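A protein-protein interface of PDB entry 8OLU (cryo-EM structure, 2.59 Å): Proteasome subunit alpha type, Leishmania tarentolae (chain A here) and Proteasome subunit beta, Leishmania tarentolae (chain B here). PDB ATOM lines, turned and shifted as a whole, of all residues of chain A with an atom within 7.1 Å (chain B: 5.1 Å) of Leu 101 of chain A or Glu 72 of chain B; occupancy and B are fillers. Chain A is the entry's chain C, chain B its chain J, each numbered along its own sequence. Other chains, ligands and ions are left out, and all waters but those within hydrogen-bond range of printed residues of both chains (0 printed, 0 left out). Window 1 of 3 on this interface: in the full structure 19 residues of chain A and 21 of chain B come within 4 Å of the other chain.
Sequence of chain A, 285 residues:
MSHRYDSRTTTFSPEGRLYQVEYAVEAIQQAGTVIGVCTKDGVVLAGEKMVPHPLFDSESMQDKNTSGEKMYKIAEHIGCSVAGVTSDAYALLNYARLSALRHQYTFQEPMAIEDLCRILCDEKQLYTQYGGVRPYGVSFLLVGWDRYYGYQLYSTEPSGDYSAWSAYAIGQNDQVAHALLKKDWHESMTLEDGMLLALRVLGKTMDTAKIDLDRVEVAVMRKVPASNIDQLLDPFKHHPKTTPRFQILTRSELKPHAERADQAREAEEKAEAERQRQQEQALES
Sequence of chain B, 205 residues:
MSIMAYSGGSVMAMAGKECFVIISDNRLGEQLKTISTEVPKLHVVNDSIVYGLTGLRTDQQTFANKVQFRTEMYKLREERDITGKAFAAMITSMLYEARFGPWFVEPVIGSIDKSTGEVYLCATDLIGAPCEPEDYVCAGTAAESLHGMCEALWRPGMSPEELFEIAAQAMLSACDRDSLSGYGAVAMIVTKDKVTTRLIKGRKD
Leu 101 of chain A touches three residues of chain B.
Of the printed residues of chain A, Glu 72 of chain B touches Leu 101 (3.9 Å).
Of the printed residues of chain A, Leu 76 of chain B touches Lys 73 (3.7 Å), Ile 74 (3.7 Å) and Arg 97 (3.8 Å).
Printed residues of chain B within 4 Å of Gln 108 of chain A: Gln 68.
Of the printed residues of chain B, Arg 97 of chain A touches Met 73 and Leu 76.
Thr 71 of chain B touches none of the printed residues of chain A.
Among the printed residues, merely in contact across the chains: Leu 101 of chain A with Met 73 of chain B, Leu 98 of chain A with Met 73 of chain B, Leu 101 of chain A with Phe 69 of chain B, Lys 73 of chain A with Leu 76 of chain B, Leu 98 of chain A with Phe 69 of chain B, Arg 97 of chain A with Met 73 of chain B, Ile 74 of chain A with Leu 76 of chain B, Arg 102 of chain A with Phe 69 of chain B, Arg 97 of chain A with Leu 76 of chain B and Leu 101 of chain A with Glu 72 of chain B.
The side-chain hydroxyl (OG1) of Thr 71 of chain B lies within hydrogen-bond range of the backbone carbonyl oxygen (O) of Gln 68 of chain B (3.4 Å).
The side-chain amino group of Lys 73 of chain A lies within salt-bridge range of the side-chain carboxylate of Glu 76 of chain A.
O of Lys 73 of chain A lies within hydrogen-bond range of NH1 of Arg 97 of chain A (2.8 Å).
The backbone carbonyl oxygen of Arg 102 of chain A is in hydrogen-bond range of the side-chain hydroxyl of Thr 106 of chain A, at 3.3 Å.
The backbone carbonyl oxygen of Gln 104 of chain A lies close to the side-chain amide nitrogen of Gln 108 of chain A.
O of Tyr 105 of chain A sits at hydrogen-bond distance from NE2 of Gln 108 of chain A, 2.8 Å away.
The side-chain amide oxygen (OE1) of Gln 108 of chain A lies within hydrogen-bond range of the side-chain amide nitrogen (NE2) of Gln 68 of chain B (3.5 Å).
Of the 10 printed residues of chain B, 5 touch a printed residue of chain A.
Hydrophobic or aromatic side chains of chain B that line the printed part of chain A: Phe 69, Met 73 and Leu 76.
Printed residues of chain A that touch a printed residue of chain B: Lys 73, Ile 74, Arg 97, Leu 98, Leu 101, Arg 102 and Gln 108.
Hydrophobic or aromatic side chains of chain A that line the printed part of chain B: Leu 98 and Leu 101.
Among the printed residues, no Asp or Glu carboxylate lies within 4 Å of a Lys or Arg side-chain nitrogen of the other chain.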
ATOM      1  N   LYS A  73     -29.102  11.368  -2.324  1.00  0.00           N
ATOM      2  CA  LYS A  73     -28.354  12.135  -1.383  1.00  0.00           C
ATOM      3  C   LYS A  73     -27.039  12.576  -1.962  1.00  0.00           C
ATOM      4  O   LYS A  73     -26.344  11.809  -2.596  1.00  0.00           O
ATOM      5  CB  LYS A  73     -28.096  11.187  -0.276  1.00  0.00           C
ATOM      6  CG  LYS A  73     -27.270  11.741   0.827  1.00  0.00           C
ATOM      7  CD  LYS A  73     -27.477  10.836   1.979  1.00  0.00           C
ATOM      8  CE  LYS A  73     -26.178  10.646   2.701  1.00  0.00           C
ATOM      9  NZ  LYS A  73     -26.498   9.848   3.909  1.00  0.00           N
ATOM     10  N   ILE A  74     -26.767  13.868  -1.845  1.00  0.00           N
ATOM     11  CA  ILE A  74     -25.500  14.456  -2.218  1.00  0.00           C
ATOM     12  C   ILE A  74     -24.519  14.498  -1.054  1.00  0.00           C
ATOM     13  O   ILE A  74     -23.327  14.435  -1.273  1.00  0.00           O
ATOM     14  CB  ILE A  74     -25.775  15.842  -2.740  1.00  0.00           C
ATOM     15  CG1 ILE A  74     -26.656  15.747  -3.962  1.00  0.00           C
ATOM     16  CG2 ILE A  74     -24.494  16.516  -3.079  1.00  0.00           C
ATOM     17  CD1 ILE A  74     -26.852  17.103  -4.648  1.00  0.00           C
ATOM     18  N   ALA A  75     -25.010  14.593   0.168  1.00  0.00           N
ATOM     19  CA  ALA A  75     -24.148  14.643   1.331  1.00  0.00           C
ATOM     20  C   ALA A  75     -25.036  14.452   2.527  1.00  0.00           C
ATOM     21  O   ALA A  75     -26.197  14.248   2.344  1.00  0.00           O
ATOM     22  CB  ALA A  75     -23.425  15.960   1.415  1.00  0.00           C
ATOM     23  N   GLU A  76     -24.497  14.456   3.731  1.00  0.00           N
ATOM     24  CA  GLU A  76     -25.358  14.169   4.862  1.00  0.00           C
ATOM     25  C   GLU A  76     -26.454  15.217   4.917  1.00  0.00           C
ATOM     26  O   GLU A  76     -27.613  14.884   5.169  1.00  0.00           O
ATOM     27  CB  GLU A  76     -24.570  14.123   6.176  1.00  0.00           C
ATOM     28  CG  GLU A  76     -23.743  12.843   6.351  1.00  0.00           C
ATOM     29  CD  GLU A  76     -24.548  11.547   6.184  1.00  0.00           C
ATOM     30  OE1 GLU A  76     -25.313  11.146   7.136  1.00  0.00           O
ATOM     31  OE2 GLU A  76     -24.443  10.945   5.082  1.00  0.00           O
ATOM     32  N   TYR A  95     -20.793  14.643  -9.783  1.00  0.00           N
ATOM     33  CA  TYR A  95     -20.083  15.892  -9.620  1.00  0.00           C
ATOM     34  C   TYR A  95     -20.485  16.639  -8.343  1.00  0.00           C
ATOM     35  O   TYR A  95     -19.663  17.171  -7.613  1.00  0.00           O
ATOM     36  CB  TYR A  95     -20.377  16.775 -10.810  1.00  0.00           C
ATOM     37  CG  TYR A  95     -19.584  18.045 -10.844  1.00  0.00           C
ATOM     38  CD1 TYR A  95     -18.216  18.037 -11.008  1.00  0.00           C
ATOM     39  CD2 TYR A  95     -20.204  19.263 -10.701  1.00  0.00           C
ATOM     40  CE1 TYR A  95     -17.476  19.217 -11.050  1.00  0.00           C
ATOM     41  CE2 TYR A  95     -19.489  20.449 -10.763  1.00  0.00           C
ATOM     42  CZ  TYR A  95     -18.119  20.435 -10.961  1.00  0.00           C
ATOM     43  OH  TYR A  95     -17.461  21.632 -11.027  1.00  0.00           O
ATOM     44  N   ALA A  96     -21.766  16.719  -8.055  1.00  0.00           N
ATOM     45  CA  ALA A  96     -22.165  17.374  -6.846  1.00  0.00           C
ATOM     46  C   ALA A  96     -21.653  16.629  -5.645  1.00  0.00           C
ATOM     47  O   ALA A  96     -21.302  17.227  -4.667  1.00  0.00           O
ATOM     48  CB  ALA A  96     -23.632  17.472  -6.778  1.00  0.00           C
ATOM     49  N   ARG A  97     -21.671  15.319  -5.655  1.00  0.00           N
ATOM     50  CA  ARG A  97     -21.103  14.588  -4.536  1.00  0.00           C
ATOM     51  C   ARG A  97     -19.653  14.909  -4.358  1.00  0.00           C
ATOM     52  O   ARG A  97     -19.263  15.177  -3.260  1.00  0.00           O
ATOM     53  CB  ARG A  97     -21.294  13.098  -4.721  1.00  0.00           C
ATOM     54  CG  ARG A  97     -22.765  12.772  -4.547  1.00  0.00           C
ATOM     55  CD  ARG A  97     -23.042  11.319  -4.754  1.00  0.00           C
ATOM     56  NE  ARG A  97     -24.406  11.030  -4.451  1.00  0.00           N
ATOM     57  CZ  ARG A  97     -24.934   9.868  -4.708  1.00  0.00           C
ATOM     58  NH1 ARG A  97     -26.039   9.476  -4.092  1.00  0.00           N
ATOM     59  NH2 ARG A  97     -24.278   9.113  -5.562  1.00  0.00           N
ATOM     60  N   LEU A  98     -18.857  14.860  -5.389  1.00  0.00           N
ATOM     61  CA  LEU A  98     -17.468  15.180  -5.171  1.00  0.00           C
ATOM     62  C   LEU A  98     -17.354  16.593  -4.682  1.00  0.00           C
ATOM     63  O   LEU A  98     -16.569  16.847  -3.804  1.00  0.00           O
ATOM     64  CB  LEU A  98     -16.664  15.109  -6.465  1.00  0.00           C
ATOM     65  CG  LEU A  98     -16.546  13.693  -6.999  1.00  0.00           C
ATOM     66  CD1 LEU A  98     -16.036  13.709  -8.453  1.00  0.00           C
ATOM     67  CD2 LEU A  98     -15.678  12.850  -6.040  1.00  0.00           C
ATOM     68  N   SER A  99     -18.023  17.530  -5.299  1.00  0.00           N
ATOM     69  CA  SER A  99     -17.862  18.875  -4.822  1.00  0.00           C
ATOM     70  C   SER A  99     -18.166  18.996  -3.324  1.00  0.00           C
ATOM     71  O   SER A  99     -17.367  19.549  -2.559  1.00  0.00           O
ATOM     72  CB  SER A  99     -18.714  19.720  -5.603  1.00  0.00           C
ATOM     73  OG  SER A  99     -18.015  19.961  -6.813  1.00  0.00           O
ATOM     74  N   ALA A 100     -19.304  18.526  -2.889  1.00  0.00           N
ATOM     75  CA  ALA A 100     -19.562  18.668  -1.503  1.00  0.00           C
ATOM     76  C   ALA A 100     -18.458  18.033  -0.665  1.00  0.00           C
ATOM     77  O   ALA A 100     -18.172  18.475   0.431  1.00  0.00           O
ATOM     78  CB  ALA A 100     -20.898  18.038  -1.211  1.00  0.00           C
ATOM     79  N   LEU A 101     -17.885  16.930  -1.080  1.00  0.00           N
ATOM     80  CA  LEU A 101     -16.859  16.327  -0.266  1.00  0.00           C
ATOM     81  C   LEU A 101     -15.505  17.009  -0.420  1.00  0.00           C
ATOM     82  O   LEU A 101     -14.711  16.993   0.513  1.00  0.00           O
ATOM     83  CB  LEU A 101     -16.713  14.874  -0.671  1.00  0.00           C
ATOM     84  CG  LEU A 101     -17.877  13.980  -0.247  1.00  0.00           C
ATOM     85  CD1 LEU A 101     -17.514  12.549  -0.435  1.00  0.00           C
ATOM     86  CD2 LEU A 101     -18.274  14.144   1.214  1.00  0.00           C
ATOM     87  N   ARG A 102     -15.216  17.605  -1.563  1.00  0.00           N
ATOM     88  CA  ARG A 102     -14.046  18.434  -1.606  1.00  0.00           C
ATOM     89  C   ARG A 102     -14.177  19.632  -0.700  1.00  0.00           C
ATOM     90  O   ARG A 102     -13.208  20.081  -0.103  1.00  0.00           O
ATOM     91  CB  ARG A 102     -13.774  18.998  -2.981  1.00  0.00           C
ATOM     92  CG  ARG A 102     -13.388  17.904  -3.951  1.00  0.00           C
ATOM     93  CD  ARG A 102     -12.904  18.528  -5.227  1.00  0.00           C
ATOM     94  NE  ARG A 102     -12.753  17.401  -6.117  1.00  0.00           N
ATOM     95  CZ  ARG A 102     -13.602  17.150  -7.096  1.00  0.00           C
ATOM     96  NH1 ARG A 102     -14.384  18.126  -7.542  1.00  0.00           N
ATOM     97  NH2 ARG A 102     -13.639  15.931  -7.613  1.00  0.00           N
ATOM     98  N   HIS A 103     -15.345  20.220  -0.649  1.00  0.00           N
ATOM     99  CA  HIS A 103     -15.489  21.303   0.290  1.00  0.00           C
ATOM    100  C   HIS A 103     -15.196  20.791   1.688  1.00  0.00           C
ATOM    101  O   HIS A 103     -14.464  21.370   2.466  1.00  0.00           O
ATOM    102  CB  HIS A 103     -16.881  21.878   0.198  1.00  0.00           C
ATOM    103  CG  HIS A 103     -17.010  23.122   0.995  1.00  0.00           C
ATOM    104  ND1 HIS A 103     -17.401  23.137   2.298  1.00  0.00           N
ATOM    105  CD2 HIS A 103     -16.579  24.367   0.646  1.00  0.00           C
ATOM    106  CE1 HIS A 103     -17.288  24.384   2.734  1.00  0.00           C
ATOM    107  NE2 HIS A 103     -16.790  25.172   1.724  1.00  0.00           N
ATOM    108  N   GLN A 104     -15.725  19.646   2.015  1.00  0.00           N
ATOM    109  CA  GLN A 104     -15.469  19.152   3.341  1.00  0.00           C
ATOM    110  C   GLN A 104     -14.018  18.766   3.530  1.00  0.00           C
ATOM    111  O   GLN A 104     -13.502  18.806   4.624  1.00  0.00           O
ATOM    112  CB  GLN A 104     -16.371  17.987   3.622  1.00  0.00           C
ATOM    113  CG  GLN A 104     -16.149  17.406   4.993  1.00  0.00           C
ATOM    114  CD  GLN A 104     -17.323  16.493   5.149  1.00  0.00           C
ATOM    115  OE1 GLN A 104     -17.221  15.309   4.785  1.00  0.00           O
ATOM    116  NE2 GLN A 104     -18.457  17.110   5.523  1.00  0.00           N
ATOM    117  N   TYR A 105     -13.337  18.379   2.480  1.00  0.00           N
ATOM    118  CA  TYR A 105     -11.936  18.054   2.626  1.00  0.00           C
ATOM    119  C   TYR A 105     -11.204  19.282   3.062  1.00  0.00           C
ATOM    120  O   TYR A 105     -10.555  19.290   4.098  1.00  0.00           O
ATOM    121  CB  TYR A 105     -11.357  17.542   1.344  1.00  0.00           C
ATOM    122  CG  TYR A 105      -9.913  17.215   1.423  1.00  0.00           C
ATOM    123  CD1 TYR A 105      -9.474  15.948   1.771  1.00  0.00           C
ATOM    124  CD2 TYR A 105      -8.958  18.160   1.090  1.00  0.00           C
ATOM    125  CE1 TYR A 105      -8.113  15.641   1.778  1.00  0.00           C
ATOM    126  CE2 TYR A 105      -7.607  17.871   1.094  1.00  0.00           C
ATOM    127  CZ  TYR A 105      -7.172  16.615   1.483  1.00  0.00           C
ATOM    128  OH  TYR A 105      -5.811  16.362   1.465  1.00  0.00           O
ATOM    129  N   THR A 106     -11.422  20.342   2.309  1.00  0.00           N
ATOM    130  CA  THR A 106     -10.703  21.573   2.481  1.00  0.00           C
ATOM    131  C   THR A 106     -11.080  22.237   3.785  1.00  0.00           C
ATOM    132  O   THR A 106     -10.202  22.437   4.603  1.00  0.00           O
ATOM    133  CB  THR A 106     -11.004  22.528   1.342  1.00  0.00           C
ATOM    134  OG1 THR A 106     -10.579  22.022   0.072  1.00  0.00           O
ATOM    135  CG2 THR A 106     -10.341  23.836   1.682  1.00  0.00           C
ATOM    136  N   PHE A 107     -12.350  22.461   4.061  1.00  0.00           N
ATOM    137  CA  PHE A 107     -12.697  23.174   5.257  1.00  0.00           C
ATOM    138  C   PHE A 107     -13.106  22.312   6.425  1.00  0.00           C
ATOM    139  O   PHE A 107     -13.277  22.784   7.525  1.00  0.00           O
ATOM    140  CB  PHE A 107     -13.873  24.046   4.932  1.00  0.00           C
ATOM    141  CG  PHE A 107     -13.515  25.047   3.868  1.00  0.00           C
ATOM    142  CD1 PHE A 107     -12.870  26.230   4.197  1.00  0.00           C
ATOM    143  CD2 PHE A 107     -13.694  24.738   2.530  1.00  0.00           C
ATOM    144  CE1 PHE A 107     -12.487  27.108   3.204  1.00  0.00           C
ATOM    145  CE2 PHE A 107     -13.245  25.587   1.526  1.00  0.00           C
ATOM    146  CZ  PHE A 107     -12.645  26.772   1.872  1.00  0.00           C
ATOM    147  N   GLN A 108     -13.340  21.033   6.257  1.00  0.00           N
ATOM    148  CA  GLN A 108     -13.852  20.239   7.353  1.00  0.00           C
ATOM    149  C   GLN A 108     -15.107  20.820   7.927  1.00  0.00           C
ATOM    150  O   GLN A 108     -15.332  20.724   9.094  1.00  0.00           O
ATOM    151  CB  GLN A 108     -12.826  20.085   8.466  1.00  0.00           C
ATOM    152  CG  GLN A 108     -11.501  19.470   7.961  1.00  0.00           C
ATOM    153  CD  GLN A 108     -11.708  18.050   7.488  1.00  0.00           C
ATOM    154  OE1 GLN A 108     -12.405  17.289   8.156  1.00  0.00           O
ATOM    155  NE2 GLN A 108     -11.129  17.700   6.339  1.00  0.00           N
ATOM    156  N   MET A 111     -20.512  21.821   3.277  1.00  0.00           N
ATOM    157  CA  MET A 111     -20.706  22.826   2.253  1.00  0.00           C
ATOM    158  C   MET A 111     -22.086  23.415   2.413  1.00  0.00           C
ATOM    159  O   MET A 111     -23.018  22.700   2.768  1.00  0.00           O
ATOM    160  CB  MET A 111     -20.686  22.146   0.893  1.00  0.00           C
ATOM    161  CG  MET A 111     -20.570  23.117  -0.190  1.00  0.00           C
ATOM    162  SD  MET A 111     -20.253  22.359  -1.738  1.00  0.00           S
ATOM    163  CE  MET A 111     -19.242  23.635  -2.483  1.00  0.00           C
ATOM    164  N   LEU A 116     -23.132  24.603  -3.106  1.00  0.00           N
ATOM    165  CA  LEU A 116     -23.184  23.349  -3.820  1.00  0.00           C
ATOM    166  C   LEU A 116     -23.952  23.617  -5.074  1.00  0.00           C
ATOM    167  O   LEU A 116     -23.531  23.321  -6.168  1.00  0.00           O
ATOM    168  CB  LEU A 116     -23.889  22.293  -2.969  1.00  0.00           C
ATOM    169  CG  LEU A 116     -23.907  20.893  -3.574  1.00  0.00           C
ATOM    170  CD1 LEU A 116     -24.979  20.800  -4.613  1.00  0.00           C
ATOM    171  CD2 LEU A 116     -22.554  20.581  -4.182  1.00  0.00           C
ATOM    172  N   VAL B  67      -8.774   9.904   3.781  1.00  0.00           N
ATOM    173  CA  VAL B  67      -9.505   8.693   3.995  1.00  0.00           C
ATOM    174  C   VAL B  67     -10.960   8.984   4.210  1.00  0.00           C
ATOM    175  O   VAL B  67     -11.810   8.250   3.776  1.00  0.00           O
ATOM    176  CB  VAL B  67      -8.939   7.909   5.170  1.00  0.00           C
ATOM    177  CG1 VAL B  67      -9.836   6.757   5.593  1.00  0.00           C
ATOM    178  CG2 VAL B  67      -7.592   7.375   4.783  1.00  0.00           C
ATOM    179  N   GLN B  68     -11.251  10.071   4.871  1.00  0.00           N
ATOM    180  CA  GLN B  68     -12.639  10.405   5.070  1.00  0.00           C
ATOM    181  C   GLN B  68     -13.306  10.857   3.780  1.00  0.00           C
ATOM    182  O   GLN B  68     -14.466  10.674   3.629  1.00  0.00           O
ATOM    183  CB  GLN B  68     -12.744  11.434   6.177  1.00  0.00           C
ATOM    184  CG  GLN B  68     -14.142  12.017   6.298  1.00  0.00           C
ATOM    185  CD  GLN B  68     -14.102  13.147   7.283  1.00  0.00           C
ATOM    186  OE1 GLN B  68     -14.431  12.931   8.461  1.00  0.00           O
ATOM    187  NE2 GLN B  68     -13.587  14.294   6.810  1.00  0.00           N
ATOM    188  N   PHE B  69     -12.612  11.411   2.831  1.00  0.00           N
ATOM    189  CA  PHE B  69     -13.242  11.698   1.564  1.00  0.00           C
ATOM    190  C   PHE B  69     -13.620  10.411   0.840  1.00  0.00           C
ATOM    191  O   PHE B  69     -14.730  10.187   0.474  1.00  0.00           O
ATOM    192  CB  PHE B  69     -12.261  12.550   0.783  1.00  0.00           C
ATOM    193  CG  PHE B  69     -12.637  12.867  -0.620  1.00  0.00           C
ATOM    194  CD1 PHE B  69     -12.566  11.924  -1.611  1.00  0.00           C
ATOM    195  CD2 PHE B  69     -13.020  14.114  -0.975  1.00  0.00           C
ATOM    196  CE1 PHE B  69     -12.938  12.215  -2.916  1.00  0.00           C
ATOM    197  CE2 PHE B  69     -13.332  14.429  -2.291  1.00  0.00           C
ATOM    198  CZ  PHE B  69     -13.310  13.475  -3.257  1.00  0.00           C
ATOM    199  N   ARG B  70     -12.638   9.553   0.646  1.00  0.00           N
ATOM    200  CA  ARG B  70     -12.793   8.237   0.112  1.00  0.00           C
ATOM    201  C   ARG B  70     -13.877   7.429   0.772  1.00  0.00           C
ATOM    202  O   ARG B  70     -14.592   6.731   0.088  1.00  0.00           O
ATOM    203  CB  ARG B  70     -11.531   7.441   0.339  1.00  0.00           C
ATOM    204  CG  ARG B  70     -10.349   7.880  -0.501  1.00  0.00           C
ATOM    205  CD  ARG B  70     -10.727   8.208  -1.914  1.00  0.00           C
ATOM    206  NE  ARG B  70     -10.821   6.942  -2.648  1.00  0.00           N
ATOM    207  CZ  ARG B  70      -9.770   6.154  -2.911  1.00  0.00           C
ATOM    208  NH1 ARG B  70      -8.497   6.582  -2.849  1.00  0.00           N
ATOM    209  NH2 ARG B  70     -10.076   4.912  -3.191  1.00  0.00           N
ATOM    210  N   THR B  71     -13.941   7.439   2.071  1.00  0.00           N
ATOM    211  CA  THR B  71     -14.933   6.596   2.667  1.00  0.00           C
ATOM    212  C   THR B  71     -16.319   7.156   2.550  1.00  0.00           C
ATOM    213  O   THR B  71     -17.227   6.374   2.535  1.00  0.00           O
ATOM    214  CB  THR B  71     -14.702   6.319   4.147  1.00  0.00           C
ATOM    215  OG1 THR B  71     -14.545   7.521   4.896  1.00  0.00           O
ATOM    216  CG2 THR B  71     -13.479   5.460   4.317  1.00  0.00           C
ATOM    217  N   GLU B  72     -16.483   8.467   2.604  1.00  0.00           N
ATOM    218  CA  GLU B  72     -17.799   9.052   2.515  1.00  0.00           C
ATOM    219  C   GLU B  72     -18.293   8.958   1.089  1.00  0.00           C
ATOM    220  O   GLU B  72     -19.459   8.692   0.858  1.00  0.00           O
ATOM    221  CB  GLU B  72     -17.829  10.514   2.922  1.00  0.00           C
ATOM    222  CG  GLU B  72     -17.626  10.781   4.422  1.00  0.00           C
ATOM    223  CD  GLU B  72     -18.688  10.316   5.436  1.00  0.00           C
ATOM    224  OE1 GLU B  72     -18.417  10.499   6.675  1.00  0.00           O
ATOM    225  OE2 GLU B  72     -19.787   9.755   5.023  1.00  0.00           O
ATOM    226  N   MET B  73     -17.371   9.046   0.152  1.00  0.00           N
ATOM    227  CA  MET B  73     -17.710   8.895  -1.234  1.00  0.00           C
ATOM    228  C   MET B  73     -18.147   7.480  -1.531  1.00  0.00           C
ATOM    229  O   MET B  73     -19.152   7.233  -2.100  1.00  0.00           O
ATOM    230  CB  MET B  73     -16.504   9.275  -2.055  1.00  0.00           C
ATOM    231  CG  MET B  73     -16.795   9.313  -3.536  1.00  0.00           C
ATOM    232  SD  MET B  73     -18.225  10.314  -4.230  1.00  0.00           S
ATOM    233  CE  MET B  73     -17.700  11.796  -3.382  1.00  0.00           C
ATOM    234  N   TYR B  74     -17.403   6.543  -1.046  1.00  0.00           N
ATOM    235  CA  TYR B  74     -17.721   5.149  -1.103  1.00  0.00           C
ATOM    236  C   TYR B  74     -19.117   4.884  -0.640  1.00  0.00           C
ATOM    237  O   TYR B  74     -19.839   4.205  -1.305  1.00  0.00           O
ATOM    238  CB  TYR B  74     -16.814   4.389  -0.164  1.00  0.00           C
ATOM    239  CG  TYR B  74     -16.922   2.902  -0.251  1.00  0.00           C
ATOM    240  CD1 TYR B  74     -17.863   2.194   0.473  1.00  0.00           C
ATOM    241  CD2 TYR B  74     -16.107   2.195  -1.096  1.00  0.00           C
ATOM    242  CE1 TYR B  74     -18.008   0.831   0.356  1.00  0.00           C
ATOM    243  CE2 TYR B  74     -16.215   0.820  -1.197  1.00  0.00           C
ATOM    244  CZ  TYR B  74     -17.172   0.144  -0.475  1.00  0.00           C
ATOM    245  OH  TYR B  74     -17.194  -1.224  -0.546  1.00  0.00           O
ATOM    246  N   LYS B  75     -19.472   5.418   0.488  1.00  0.00           N
ATOM    247  CA  LYS B  75     -20.741   5.143   1.122  1.00  0.00           C
ATOM    248  C   LYS B  75     -21.867   5.762   0.317  1.00  0.00           C
ATOM    249  O   LYS B  75     -22.959   5.233   0.291  1.00  0.00           O
ATOM    250  CB  LYS B  75     -20.566   5.605   2.573  1.00  0.00           C
ATOM    251  CG  LYS B  75     -21.807   5.964   3.332  1.00  0.00           C
ATOM    252  CD  LYS B  75     -22.181   4.960   4.341  1.00  0.00           C
ATOM    253  CE  LYS B  75     -23.468   5.319   5.054  1.00  0.00           C
ATOM    254  NZ  LYS B  75     -24.141   4.083   5.533  1.00  0.00           N
ATOM    255  N   LEU B  76     -21.630   6.855  -0.375  1.00  0.00           N
ATOM    256  CA  LEU B  76     -22.671   7.382  -1.229  1.00  0.00           C
ATOM    257  C   LEU B  76     -22.828   6.589  -2.514  1.00  0.00           C
ATOM    258  O   LEU B  76     -23.930   6.341  -2.964  1.00  0.00           O
ATOM    259  CB  LEU B  76     -22.325   8.806  -1.621  1.00  0.00           C
ATOM    260  CG  LEU B  76     -22.504   9.833  -0.514  1.00  0.00           C
ATOM    261  CD1 LEU B  76     -21.722  11.094  -0.810  1.00  0.00           C
ATOM    262  CD2 LEU B  76     -23.937  10.185  -0.322  1.00  0.00           C
